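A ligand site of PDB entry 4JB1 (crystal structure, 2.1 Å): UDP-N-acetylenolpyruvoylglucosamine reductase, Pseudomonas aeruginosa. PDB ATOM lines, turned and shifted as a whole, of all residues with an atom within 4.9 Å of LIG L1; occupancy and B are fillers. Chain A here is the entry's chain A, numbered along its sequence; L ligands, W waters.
N7 of LG2 L2 sits at hydrogen-bond distance from O of Gly 131.
An oxygen (O14) of LIG L1 is in hydrogen-bond range of the backbone NH (N) of Ser 240.
The guanidinium group (NE) of Arg 167 is in hydrogen-bond range of an oxygen (O7) of LG2 L2 (3.4 Å).
The side-chain amino group of Lys 273 is in salt-bridge range of an oxygen (O16) of LIG L1, at 2.5 Å.
The side-chain hydroxyl (OH) of Tyr 197 is in hydrogen-bond range of an oxygen (O17) of LIG L1.
The guanidinium group (NH1) of Arg 225 is in hydrogen-bond range of an oxygen (O8) of LG2 L2 (2.9 Å).
NH2 of Arg 167 lies within hydrogen-bond range of O13 of LIG L1 (3.2 Å).
The side-chain amino group (NZ) of Lys 228 lies within salt-bridge range of an oxygen (O8) of LIG L1 (2.7 Å).
A nitrogen (N3) of LIG L1 is in hydrogen-bond range of the backbone carbonyl oxygen of Asp 196 (3.5 Å).
N7 of LIG L1 is in hydrogen-bond range of OE2 of Glu 336 (2.9 Å).
N of Tyr 133 lies within hydrogen-bond range of O12 of LIG L1.
The side-chain hydroxyl of Tyr 265 sits close to an oxygen (O4) of LIG L1 (3.5 Å).
The backbone NH (N) of Gly 131 is in hydrogen-bond range of an oxygen (O7) of LG2 L2 (3.1 Å).
ND2 of Asn 244 is in hydrogen-bond range of O5 of LIG L1, at 2.8 Å.
O of Lys 273 sits at hydrogen-bond distance from N of Tyr 265, at 2.8 Å.
OE1 of Glu 336 lies within salt-bridge range of NE of Arg 167, 2.9 Å away.
The backbone NH of Ala 276 lies within hydrogen-bond range of the side-chain amide oxygen of Asn 244 (2.9 Å).
N of Asn 244 lies within hydrogen-bond range of OH of Tyr 166, at 2.9 Å.
NH2 of Arg 167 lies within hydrogen-bond range of O of Gly 131 (3.2 Å).
Ala 132 touches LIG L1.
NH1 of Arg 225 touches C21 of LIG L1 (3.6 Å).
Leu 229 touches LIG L1.
CA of Gly 239 touches O14 of LIG L1, 3.8 Å away.
Ala 275 touches LIG L1.
Hydrophobic or aromatic side chains that line LIG L1: Ala 132, Tyr 133, Tyr 197, Leu 229, Tyr 265 and Ala 275.
Within 4 Å of LIG L1: Ala 132, Tyr 133, Arg 167, Asp 196, Tyr 197, Arg 225, Lys 228, Leu 229, Gly 239, Ser 240, Asn 244, Tyr 265, Lys 273, Ala 275 and Glu 336.
The nearest printed residue that does not touch LIG L1 is Gly 131 (4.1 Å).
Water W5 bridges an oxygen (O9) of LIG L1 (2.7 Å) and the side-chain amide oxygen (OE1) of Gln 299 (2.9 Å).
Water W6 bridges N7 of LIG L1 (2.8 Å) and NH2 of Arg 167 (3.1 Å).
Water W1 bridges OH of Tyr 265 (2.7 Å) and O4 of LIG L1 (3.1 Å).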
ATOM      1  N   GLY A 131     -30.841 -12.328  20.456  1.00  0.00           N
ATOM      2  CA  GLY A 131     -30.880 -11.845  19.064  1.00  0.00           C
ATOM      3  C   GLY A 131     -29.752 -12.453  18.192  1.00  0.00           C
ATOM      4  O   GLY A 131     -28.693 -12.854  18.698  1.00  0.00           O
ATOM      5  N   ALA A 132     -30.052 -12.539  16.884  1.00  0.00           N
ATOM      6  CA  ALA A 132     -29.108 -12.992  15.873  1.00  0.00           C
ATOM      7  C   ALA A 132     -29.707 -12.541  14.532  1.00  0.00           C
ATOM      8  O   ALA A 132     -30.935 -12.506  14.350  1.00  0.00           O
ATOM      9  CB  ALA A 132     -28.881 -14.515  15.929  1.00  0.00           C
ATOM     10  N   TYR A 133     -28.837 -12.022  13.684  1.00  0.00           N
ATOM     11  CA  TYR A 133     -29.099 -11.874  12.271  1.00  0.00           C
ATOM     12  C   TYR A 133     -30.142 -10.861  11.994  1.00  0.00           C
ATOM     13  O   TYR A 133     -30.869 -11.026  11.025  1.00  0.00           O
ATOM     14  CB  TYR A 133     -29.432 -13.215  11.645  1.00  0.00           C
ATOM     15  CG  TYR A 133     -28.180 -14.087  11.602  1.00  0.00           C
ATOM     16  CD1 TYR A 133     -27.083 -13.783  10.772  1.00  0.00           C
ATOM     17  CD2 TYR A 133     -28.064 -15.200  12.354  1.00  0.00           C
ATOM     18  CE1 TYR A 133     -25.942 -14.605  10.706  1.00  0.00           C
ATOM     19  CE2 TYR A 133     -26.915 -16.050  12.277  1.00  0.00           C
ATOM     20  CZ  TYR A 133     -25.847 -15.707  11.476  1.00  0.00           C
ATOM     21  OH  TYR A 133     -24.735 -16.543  11.413  1.00  0.00           O
ATOM     22  N   GLY A 134     -30.174  -9.814  12.821  1.00  0.00           N
ATOM     23  CA  GLY A 134     -31.112  -8.689  12.592  1.00  0.00           C
ATOM     24  C   GLY A 134     -32.464  -8.827  13.301  1.00  0.00           C
ATOM     25  O   GLY A 134     -33.298  -7.951  13.226  1.00  0.00           O
ATOM     26  N   TYR A 166     -30.583  -3.923  24.102  1.00  0.00           N
ATOM     27  CA  TYR A 166     -29.645  -4.759  23.477  1.00  0.00           C
ATOM     28  C   TYR A 166     -29.021  -5.652  24.504  1.00  0.00           C
ATOM     29  O   TYR A 166     -28.322  -5.220  25.415  1.00  0.00           O
ATOM     30  CB  TYR A 166     -28.589  -3.960  22.718  1.00  0.00           C
ATOM     31  CG  TYR A 166     -27.382  -4.782  22.127  1.00  0.00           C
ATOM     32  CD1 TYR A 166     -27.534  -5.730  21.180  1.00  0.00           C
ATOM     33  CD2 TYR A 166     -26.117  -4.492  22.513  1.00  0.00           C
ATOM     34  CE1 TYR A 166     -26.440  -6.421  20.643  1.00  0.00           C
ATOM     35  CE2 TYR A 166     -25.015  -5.158  21.991  1.00  0.00           C
ATOM     36  CZ  TYR A 166     -25.175  -6.088  21.045  1.00  0.00           C
ATOM     37  OH  TYR A 166     -24.038  -6.721  20.602  1.00  0.00           O
ATOM     38  N   ARG A 167     -29.191  -6.913  24.301  1.00  0.00           N
ATOM     39  CA  ARG A 167     -28.808  -7.935  25.232  1.00  0.00           C
ATOM     40  C   ARG A 167     -29.179  -7.565  26.685  1.00  0.00           C
ATOM     41  O   ARG A 167     -28.409  -7.763  27.597  1.00  0.00           O
ATOM     42  CB  ARG A 167     -27.324  -8.261  25.101  1.00  0.00           C
ATOM     43  CG  ARG A 167     -26.922  -8.836  23.772  1.00  0.00           C
ATOM     44  CD  ARG A 167     -27.658 -10.158  23.506  1.00  0.00           C
ATOM     45  NE  ARG A 167     -27.051 -10.668  22.310  1.00  0.00           N
ATOM     46  CZ  ARG A 167     -27.383 -10.353  21.069  1.00  0.00           C
ATOM     47  NH1 ARG A 167     -28.389  -9.578  20.797  1.00  0.00           N
ATOM     48  NH2 ARG A 167     -26.623 -10.827  20.087  1.00  0.00           N
ATOM     49  N   ASP A 196     -31.286  -8.950   6.004  1.00  0.00           N
ATOM     50  CA  ASP A 196     -30.269  -7.932   6.013  1.00  0.00           C
ATOM     51  C   ASP A 196     -28.829  -8.440   6.146  1.00  0.00           C
ATOM     52  O   ASP A 196     -27.950  -7.736   5.741  1.00  0.00           O
ATOM     53  CB  ASP A 196     -30.507  -6.968   7.128  1.00  0.00           C
ATOM     54  CG  ASP A 196     -31.641  -6.085   6.831  1.00  0.00           C
ATOM     55  OD1 ASP A 196     -32.289  -6.330   5.795  1.00  0.00           O
ATOM     56  OD2 ASP A 196     -31.839  -5.134   7.601  1.00  0.00           O
ATOM     57  N   TYR A 197     -28.592  -9.597   6.752  1.00  0.00           N
ATOM     58  CA  TYR A 197     -27.219 -10.061   6.919  1.00  0.00           C
ATOM     59  C   TYR A 197     -26.779 -10.788   5.661  1.00  0.00           C
ATOM     60  O   TYR A 197     -27.367 -11.812   5.278  1.00  0.00           O
ATOM     61  CB  TYR A 197     -27.033 -10.940   8.136  1.00  0.00           C
ATOM     62  CG  TYR A 197     -27.021 -10.135   9.417  1.00  0.00           C
ATOM     63  CD1 TYR A 197     -28.022  -9.218   9.707  1.00  0.00           C
ATOM     64  CD2 TYR A 197     -26.063 -10.336  10.357  1.00  0.00           C
ATOM     65  CE1 TYR A 197     -28.017  -8.467  10.921  1.00  0.00           C
ATOM     66  CE2 TYR A 197     -26.061  -9.619  11.556  1.00  0.00           C
ATOM     67  CZ  TYR A 197     -27.042  -8.692  11.846  1.00  0.00           C
ATOM     68  OH  TYR A 197     -27.020  -7.988  13.048  1.00  0.00           O
ATOM     69  N   ARG A 225     -24.104 -21.320  11.345  1.00  0.00           N
ATOM     70  CA  ARG A 225     -23.765 -21.422  12.762  1.00  0.00           C
ATOM     71  C   ARG A 225     -22.975 -22.732  13.070  1.00  0.00           C
ATOM     72  O   ARG A 225     -21.987 -22.694  13.799  1.00  0.00           O
ATOM     73  CB  ARG A 225     -25.048 -21.318  13.628  1.00  0.00           C
ATOM     74  CG  ARG A 225     -25.707 -19.918  13.569  1.00  0.00           C
ATOM     75  CD  ARG A 225     -26.877 -19.799  14.505  1.00  0.00           C
ATOM     76  NE  ARG A 225     -26.477 -19.872  15.924  1.00  0.00           N
ATOM     77  CZ  ARG A 225     -26.510 -18.897  16.827  1.00  0.00           C
ATOM     78  NH1 ARG A 225     -26.909 -17.680  16.515  1.00  0.00           N
ATOM     79  NH2 ARG A 225     -26.065 -19.115  18.070  1.00  0.00           N
ATOM     80  N   LYS A 228     -19.358 -22.385  11.682  1.00  0.00           N
ATOM     81  CA  LYS A 228     -18.390 -21.485  12.278  1.00  0.00           C
ATOM     82  C   LYS A 228     -18.299 -21.400  13.801  1.00  0.00           C
ATOM     83  O   LYS A 228     -17.312 -20.907  14.324  1.00  0.00           O
ATOM     84  CB  LYS A 228     -18.512 -20.084  11.655  1.00  0.00           C
ATOM     85  CG  LYS A 228     -19.696 -19.259  12.026  1.00  0.00           C
ATOM     86  CD  LYS A 228     -19.760 -18.034  11.126  1.00  0.00           C
ATOM     87  CE  LYS A 228     -18.946 -16.905  11.692  1.00  0.00           C
ATOM     88  NZ  LYS A 228     -19.422 -15.630  11.119  1.00  0.00           N
ATOM     89  N   LEU A 229     -19.253 -21.951  14.525  1.00  0.00           N
ATOM     90  CA  LEU A 229     -19.320 -21.689  15.937  1.00  0.00           C
ATOM     91  C   LEU A 229     -18.905 -22.855  16.764  1.00  0.00           C
ATOM     92  O   LEU A 229     -19.603 -23.899  16.729  1.00  0.00           O
ATOM     93  CB  LEU A 229     -20.743 -21.324  16.399  1.00  0.00           C
ATOM     94  CG  LEU A 229     -21.383 -20.172  15.695  1.00  0.00           C
ATOM     95  CD1 LEU A 229     -22.701 -19.885  16.408  1.00  0.00           C
ATOM     96  CD2 LEU A 229     -20.483 -18.965  15.685  1.00  0.00           C
ATOM     97  N   ALA A 238     -19.293 -19.746  26.109  1.00  0.00           N
ATOM     98  CA  ALA A 238     -20.667 -19.219  26.318  1.00  0.00           C
ATOM     99  C   ALA A 238     -20.948 -18.278  25.167  1.00  0.00           C
ATOM    100  O   ALA A 238     -21.659 -17.294  25.321  1.00  0.00           O
ATOM    101  CB  ALA A 238     -20.781 -18.523  27.680  1.00  0.00           C
ATOM    102  N   GLY A 239     -20.389 -18.579  23.985  1.00  0.00           N
ATOM    103  CA  GLY A 239     -20.781 -17.911  22.832  1.00  0.00           C
ATOM    104  C   GLY A 239     -19.955 -16.647  22.781  1.00  0.00           C
ATOM    105  O   GLY A 239     -18.829 -16.617  23.263  1.00  0.00           O
ATOM    106  N   SER A 240     -20.545 -15.612  22.181  1.00  0.00           N
ATOM    107  CA  SER A 240     -19.961 -14.293  22.095  1.00  0.00           C
ATOM    108  C   SER A 240     -19.852 -13.726  23.477  1.00  0.00           C
ATOM    109  O   SER A 240     -20.873 -13.571  24.111  1.00  0.00           O
ATOM    110  CB  SER A 240     -20.770 -13.413  21.151  1.00  0.00           C
ATOM    111  OG  SER A 240     -20.461 -13.822  19.829  1.00  0.00           O
ATOM    112  N   ASN A 244     -21.389  -5.929  21.501  1.00  0.00           N
ATOM    113  CA  ASN A 244     -20.930  -4.788  20.725  1.00  0.00           C
ATOM    114  C   ASN A 244     -21.121  -3.455  21.449  1.00  0.00           C
ATOM    115  O   ASN A 244     -22.178  -3.156  21.816  1.00  0.00           O
ATOM    116  CB  ASN A 244     -21.669  -4.749  19.425  1.00  0.00           C
ATOM    117  CG  ASN A 244     -21.271  -5.873  18.515  1.00  0.00           C
ATOM    118  OD1 ASN A 244     -20.145  -6.376  18.543  1.00  0.00           O
ATOM    119  ND2 ASN A 244     -22.208  -6.291  17.706  1.00  0.00           N
ATOM    120  N   TYR A 265     -21.740   0.185  12.802  1.00  0.00           N
ATOM    121  CA  TYR A 265     -23.028   0.213  12.130  1.00  0.00           C
ATOM    122  C   TYR A 265     -23.836   1.356  12.710  1.00  0.00           C
ATOM    123  O   TYR A 265     -24.136   1.303  13.883  1.00  0.00           O
ATOM    124  CB  TYR A 265     -23.749  -1.112  12.352  1.00  0.00           C
ATOM    125  CG  TYR A 265     -23.066  -2.293  11.634  1.00  0.00           C
ATOM    126  CD1 TYR A 265     -22.003  -2.975  12.231  1.00  0.00           C
ATOM    127  CD2 TYR A 265     -23.480  -2.699  10.341  1.00  0.00           C
ATOM    128  CE1 TYR A 265     -21.381  -4.012  11.584  1.00  0.00           C
ATOM    129  CE2 TYR A 265     -22.849  -3.743   9.681  1.00  0.00           C
ATOM    130  CZ  TYR A 265     -21.795  -4.376  10.309  1.00  0.00           C
ATOM    131  OH  TYR A 265     -21.189  -5.410   9.680  1.00  0.00           O
ATOM    132  N   LYS A 273     -22.732   1.562  16.523  1.00  0.00           N
ATOM    133  CA  LYS A 273     -22.537   0.221  17.107  1.00  0.00           C
ATOM    134  C   LYS A 273     -21.274  -0.333  16.531  1.00  0.00           C
ATOM    135  O   LYS A 273     -21.272  -0.766  15.402  1.00  0.00           O
ATOM    136  CB  LYS A 273     -23.707  -0.772  16.820  1.00  0.00           C
ATOM    137  CG  LYS A 273     -23.424  -2.222  17.325  1.00  0.00           C
ATOM    138  CD  LYS A 273     -24.557  -3.218  17.012  1.00  0.00           C
ATOM    139  CE  LYS A 273     -24.644  -3.513  15.529  1.00  0.00           C
ATOM    140  NZ  LYS A 273     -25.147  -4.858  15.241  1.00  0.00           N
ATOM    141  N   ALA A 275     -18.211  -3.160  16.066  1.00  0.00           N
ATOM    142  CA  ALA A 275     -18.111  -4.617  16.057  1.00  0.00           C
ATOM    143  C   ALA A 275     -17.040  -4.999  17.017  1.00  0.00           C
ATOM    144  O   ALA A 275     -15.867  -4.668  16.799  1.00  0.00           O
ATOM    145  CB  ALA A 275     -17.734  -5.111  14.663  1.00  0.00           C
ATOM    146  N   ALA A 276     -17.411  -5.718  18.070  1.00  0.00           N
ATOM    147  CA  ALA A 276     -16.426  -6.101  19.101  1.00  0.00           C
ATOM    148  C   ALA A 276     -15.413  -7.142  18.614  1.00  0.00           C
ATOM    149  O   ALA A 276     -14.265  -7.202  19.099  1.00  0.00           O
ATOM    150  CB  ALA A 276     -17.133  -6.602  20.337  1.00  0.00           C
ATOM    151  N   GLN A 299     -13.212 -17.088  15.678  1.00  0.00           N
ATOM    152  CA  GLN A 299     -14.248 -16.245  16.334  1.00  0.00           C
ATOM    153  C   GLN A 299     -13.700 -15.472  17.550  1.00  0.00           C
ATOM    154  O   GLN A 299     -13.662 -15.961  18.668  1.00  0.00           O
ATOM    155  CB  GLN A 299     -15.479 -17.120  16.674  1.00  0.00           C
ATOM    156  CG  GLN A 299     -15.943 -18.093  15.570  1.00  0.00           C
ATOM    157  CD  GLN A 299     -16.219 -17.384  14.273  1.00  0.00           C
ATOM    158  OE1 GLN A 299     -16.960 -16.444  14.226  1.00  0.00           O
ATOM    159  NE2 GLN A 299     -15.565 -17.835  13.202  1.00  0.00           N
ATOM    160  N   GLU A 336     -21.444 -10.525  27.990  1.00  0.00           N
ATOM    161  CA  GLU A 336     -22.728 -11.091  27.804  1.00  0.00           C
ATOM    162  C   GLU A 336     -23.111 -12.085  28.901  1.00  0.00           C
ATOM    163  O   GLU A 336     -24.171 -11.987  29.450  1.00  0.00           O
ATOM    164  CB  GLU A 336     -22.848 -11.674  26.408  1.00  0.00           C
ATOM    165  CG  GLU A 336     -24.275 -11.838  25.999  1.00  0.00           C
ATOM    166  CD  GLU A 336     -24.409 -12.315  24.583  1.00  0.00           C
ATOM    167  OE1 GLU A 336     -24.642 -11.490  23.680  1.00  0.00           O
ATOM    168  OE2 GLU A 336     -24.331 -13.549  24.388  1.00  0.00           O
HETATM  169  P1  LIG L   1     -21.227 -11.684  11.926  1.00  0.00           P
HETATM  170  O1  LIG L   1     -19.892 -12.025  11.312  1.00  0.00           O
HETATM  171  O2  LIG L   1     -22.498 -11.954  11.210  1.00  0.00           O
HETATM  172  O3  LIG L   1     -21.241 -10.123  12.135  1.00  0.00           O
HETATM  173  C1  LIG L   1     -20.067  -9.616  12.773  1.00  0.00           C
HETATM  174  C2  LIG L   1     -20.339  -8.293  13.424  1.00  0.00           C
HETATM  175  O4  LIG L   1     -20.964  -7.461  12.483  1.00  0.00           O
HETATM  176  C3  LIG L   1     -21.340  -8.420  14.595  1.00  0.00           C
HETATM  177  O5  LIG L   1     -20.867  -7.381  15.444  1.00  0.00           O
HETATM  178  C4  LIG L   1     -22.728  -8.135  14.029  1.00  0.00           C
HETATM  179  O6  LIG L   1     -23.637  -7.464  14.984  1.00  0.00           O
HETATM  180  C5  LIG L   1     -22.331  -7.186  12.867  1.00  0.00           C
HETATM  181  N1  LIG L   1     -23.140  -7.194  11.627  1.00  0.00           N
HETATM  182  C6  LIG L   1     -23.011  -7.966  10.511  1.00  0.00           C
HETATM  183  N2  LIG L   1     -23.950  -7.635   9.567  1.00  0.00           N
HETATM  184  C7  LIG L   1     -24.697  -6.672  10.113  1.00  0.00           C
HETATM  185  C8  LIG L   1     -25.791  -5.878   9.612  1.00  0.00           C
HETATM  186  N3  LIG L   1     -26.252  -6.154   8.356  1.00  0.00           N
HETATM  187  N4  LIG L   1     -26.295  -4.977  10.479  1.00  0.00           N
HETATM  188  C9  LIG L   1     -25.763  -4.765  11.691  1.00  0.00           C
HETATM  189  N5  LIG L   1     -24.700  -5.439  12.177  1.00  0.00           N
HETATM  190  C10 LIG L   1     -24.184  -6.377  11.443  1.00  0.00           C
HETATM  191  O7  LIG L   1     -21.107 -12.160  13.436  1.00  0.00           O
HETATM  192  P2  LIG L   1     -21.351 -13.606  13.995  1.00  0.00           P
HETATM  193  O8  LIG L   1     -21.108 -14.280  12.716  1.00  0.00           O
HETATM  194  O9  LIG L   1     -20.618 -13.781  15.293  1.00  0.00           O
HETATM  195  O10 LIG L   1     -22.901 -13.804  14.546  1.00  0.00           O
HETATM  196  C11 LIG L   1     -24.043 -13.837  13.664  1.00  0.00           C
HETATM  197  C12 LIG L   1     -25.308 -13.293  14.373  1.00  0.00           C
HETATM  198  O11 LIG L   1     -25.607 -14.147  15.458  1.00  0.00           O
HETATM  199  C13 LIG L   1     -25.061 -11.943  14.937  1.00  0.00           C
HETATM  200  O12 LIG L   1     -26.243 -11.224  14.772  1.00  0.00           O
HETATM  201  C14 LIG L   1     -24.613 -12.227  16.365  1.00  0.00           C
HETATM  202  O13 LIG L   1     -25.094 -11.301  17.350  1.00  0.00           O
HETATM  203  C15 LIG L   1     -25.237 -13.523  16.662  1.00  0.00           C
HETATM  204  N6  LIG L   1     -24.510 -14.496  17.447  1.00  0.00           N
HETATM  205  C16 LIG L   1     -24.486 -14.250  18.733  1.00  0.00           C
HETATM  206  C17 LIG L   1     -23.938 -15.116  19.636  1.00  0.00           C
HETATM  207  C18 LIG L   1     -23.970 -14.719  21.081  1.00  0.00           C
HETATM  208  O14 LIG L   1     -23.641 -15.589  21.838  1.00  0.00           O
HETATM  209  N7  LIG L   1     -24.337 -13.479  21.488  1.00  0.00           N
HETATM  210  C19 LIG L   1     -23.376 -16.304  19.180  1.00  0.00           C
HETATM  211  C20 LIG L   1     -23.420 -16.554  17.803  1.00  0.00           C
HETATM  212  C21 LIG L   1     -23.998 -15.638  16.940  1.00  0.00           C
HETATM  213  P3  LIG L   1     -24.729  -8.188  15.869  1.00  0.00           P
HETATM  214  O15 LIG L   1     -23.975  -9.134  16.759  1.00  0.00           O
HETATM  215  O16 LIG L   1     -25.299  -6.945  16.607  1.00  0.00           O
HETATM  216  O17 LIG L   1     -25.679  -8.956  14.906  1.00  0.00           O
HETATM  217  P1  LG2 L   2     -28.673 -19.677  31.567  1.00  0.00           P
HETATM  218  O1  LG2 L   2     -29.213 -20.941  32.131  1.00  0.00           O
HETATM  219  O2  LG2 L   2     -27.268 -19.570  31.026  1.00  0.00           O
HETATM  220  O3  LG2 L   2     -29.179 -18.391  32.447  1.00  0.00           O
HETATM  221  C1  LG2 L   2     -28.865 -17.056  32.037  1.00  0.00           C
HETATM  222  C2  LG2 L   2     -29.389 -16.050  33.019  1.00  0.00           C
HETATM  223  O4  LG2 L   2     -30.858 -16.064  33.037  1.00  0.00           O
HETATM  224  C3  LG2 L   2     -28.950 -16.481  34.427  1.00  0.00           C
HETATM  225  O5  LG2 L   2     -28.788 -15.289  35.104  1.00  0.00           O
HETATM  226  C4  LG2 L   2     -30.124 -17.214  35.019  1.00  0.00           C
HETATM  227  O6  LG2 L   2     -30.198 -17.065  36.428  1.00  0.00           O
HETATM  228  C5  LG2 L   2     -31.289 -16.508  34.342  1.00  0.00           C
HETATM  229  N1  LG2 L   2     -32.490 -17.353  34.115  1.00  0.00           N
HETATM  230  C6  LG2 L   2     -32.502 -18.471  33.372  1.00  0.00           C
HETATM  231  N2  LG2 L   2     -33.735 -18.968  33.331  1.00  0.00           N
HETATM  232  C7  LG2 L   2     -34.495 -18.111  34.062  1.00  0.00           C
HETATM  233  C8  LG2 L   2     -35.875 -18.028  34.402  1.00  0.00           C
HETATM  234  N3  LG2 L   2     -36.653 -18.984  34.005  1.00  0.00           N
HETATM  235  N4  LG2 L   2     -36.315 -17.009  35.125  1.00  0.00           N
HETATM  236  C9  LG2 L   2     -35.452 -16.085  35.610  1.00  0.00           C
HETATM  237  N5  LG2 L   2     -34.130 -16.110  35.310  1.00  0.00           N
HETATM  238  C10 LG2 L   2     -33.671 -17.073  34.560  1.00  0.00           C
HETATM  239  N6  LG2 L   2     -27.356 -15.416  22.702  1.00  0.00           N
HETATM  240  C11 LG2 L   2     -27.944 -14.603  21.813  1.00  0.00           C
HETATM  241  O7  LG2 L   2     -28.677 -13.682  22.271  1.00  0.00           O
HETATM  242  N7  LG2 L   2     -27.765 -14.784  20.483  1.00  0.00           N
HETATM  243  C12 LG2 L   2     -27.010 -15.757  19.968  1.00  0.00           C
HETATM  244  O8  LG2 L   2     -26.845 -15.885  18.736  1.00  0.00           O
HETATM  245  C13 LG2 L   2     -26.335 -16.665  20.909  1.00  0.00           C
HETATM  246  N8  LG2 L   2     -25.504 -17.575  20.484  1.00  0.00           N
HETATM  247  C14 LG2 L   2     -24.935 -18.461  21.337  1.00  0.00           C
HETATM  248  C15 LG2 L   2     -24.077 -19.499  20.862  1.00  0.00           C
HETATM  249  C16 LG2 L   2     -23.411 -20.354  21.767  1.00  0.00           C
HETATM  250  C17 LG2 L   2     -22.523 -21.501  21.317  1.00  0.00           C
HETATM  251  C18 LG2 L   2     -23.611 -20.191  23.229  1.00  0.00           C
HETATM  252  C19 LG2 L   2     -22.952 -21.144  24.217  1.00  0.00           C
HETATM  253  C20 LG2 L   2     -24.477 -19.156  23.685  1.00  0.00           C
HETATM  254  C21 LG2 L   2     -25.099 -18.259  22.789  1.00  0.00           C
HETATM  255  N9  LG2 L   2     -25.937 -17.200  23.251  1.00  0.00           N
HETATM  256  C22 LG2 L   2     -26.536 -16.401  22.325  1.00  0.00           C
HETATM  257  C23 LG2 L   2     -26.178 -16.986  24.658  1.00  0.00           C
HETATM  258  C24 LG2 L   2     -27.264 -17.877  25.245  1.00  0.00           C
HETATM  259  O9  LG2 L   2     -27.598 -19.021  24.471  1.00  0.00           O
HETATM  260  C25 LG2 L   2     -28.581 -17.093  25.482  1.00  0.00           C
HETATM  261  O10 LG2 L   2     -28.193 -15.989  26.250  1.00  0.00           O
HETATM  262  C26 LG2 L   2     -29.666 -17.881  26.197  1.00  0.00           C
HETATM  263  O11 LG2 L   2     -30.851 -17.163  26.364  1.00  0.00           O
HETATM  264  C27 LG2 L   2     -29.346 -18.336  27.639  1.00  0.00           C
HETATM  265  O12 LG2 L   2     -30.313 -19.341  27.958  1.00  0.00           O
HETATM  266  P2  LG2 L   2     -30.050 -20.458  29.141  1.00  0.00           P
HETATM  267  O13 LG2 L   2     -31.426 -21.103  29.326  1.00  0.00           O
HETATM  268  O14 LG2 L   2     -28.874 -21.206  28.708  1.00  0.00           O
HETATM  269  O15 LG2 L   2     -29.690 -19.351  30.317  1.00  0.00           O
HETATM  270  O   HOH W   1     -19.138  -7.052  10.043  1.00  0.00           O
HETATM  271  O   HOH W   2     -20.829 -18.423  19.392  1.00  0.00           O
HETATM  272  O   HOH W   3     -23.383 -10.610   8.903  1.00  0.00           O
HETATM  273  O   HOH W   4     -18.190  -8.803  16.240  1.00  0.00           O
HETATM  274  O   HOH W   5     -18.599 -15.267  16.254  1.00  0.00           O
HETATM  275  O   HOH W   6     -23.551 -11.022  20.333  1.00  0.00           O
HETATM  276  O   HOH W   7     -24.549  -7.729   6.618  1.00  0.00           O
HETATM  277  O   HOH W   8     -28.807  -3.702   9.718  1.00  0.00           O
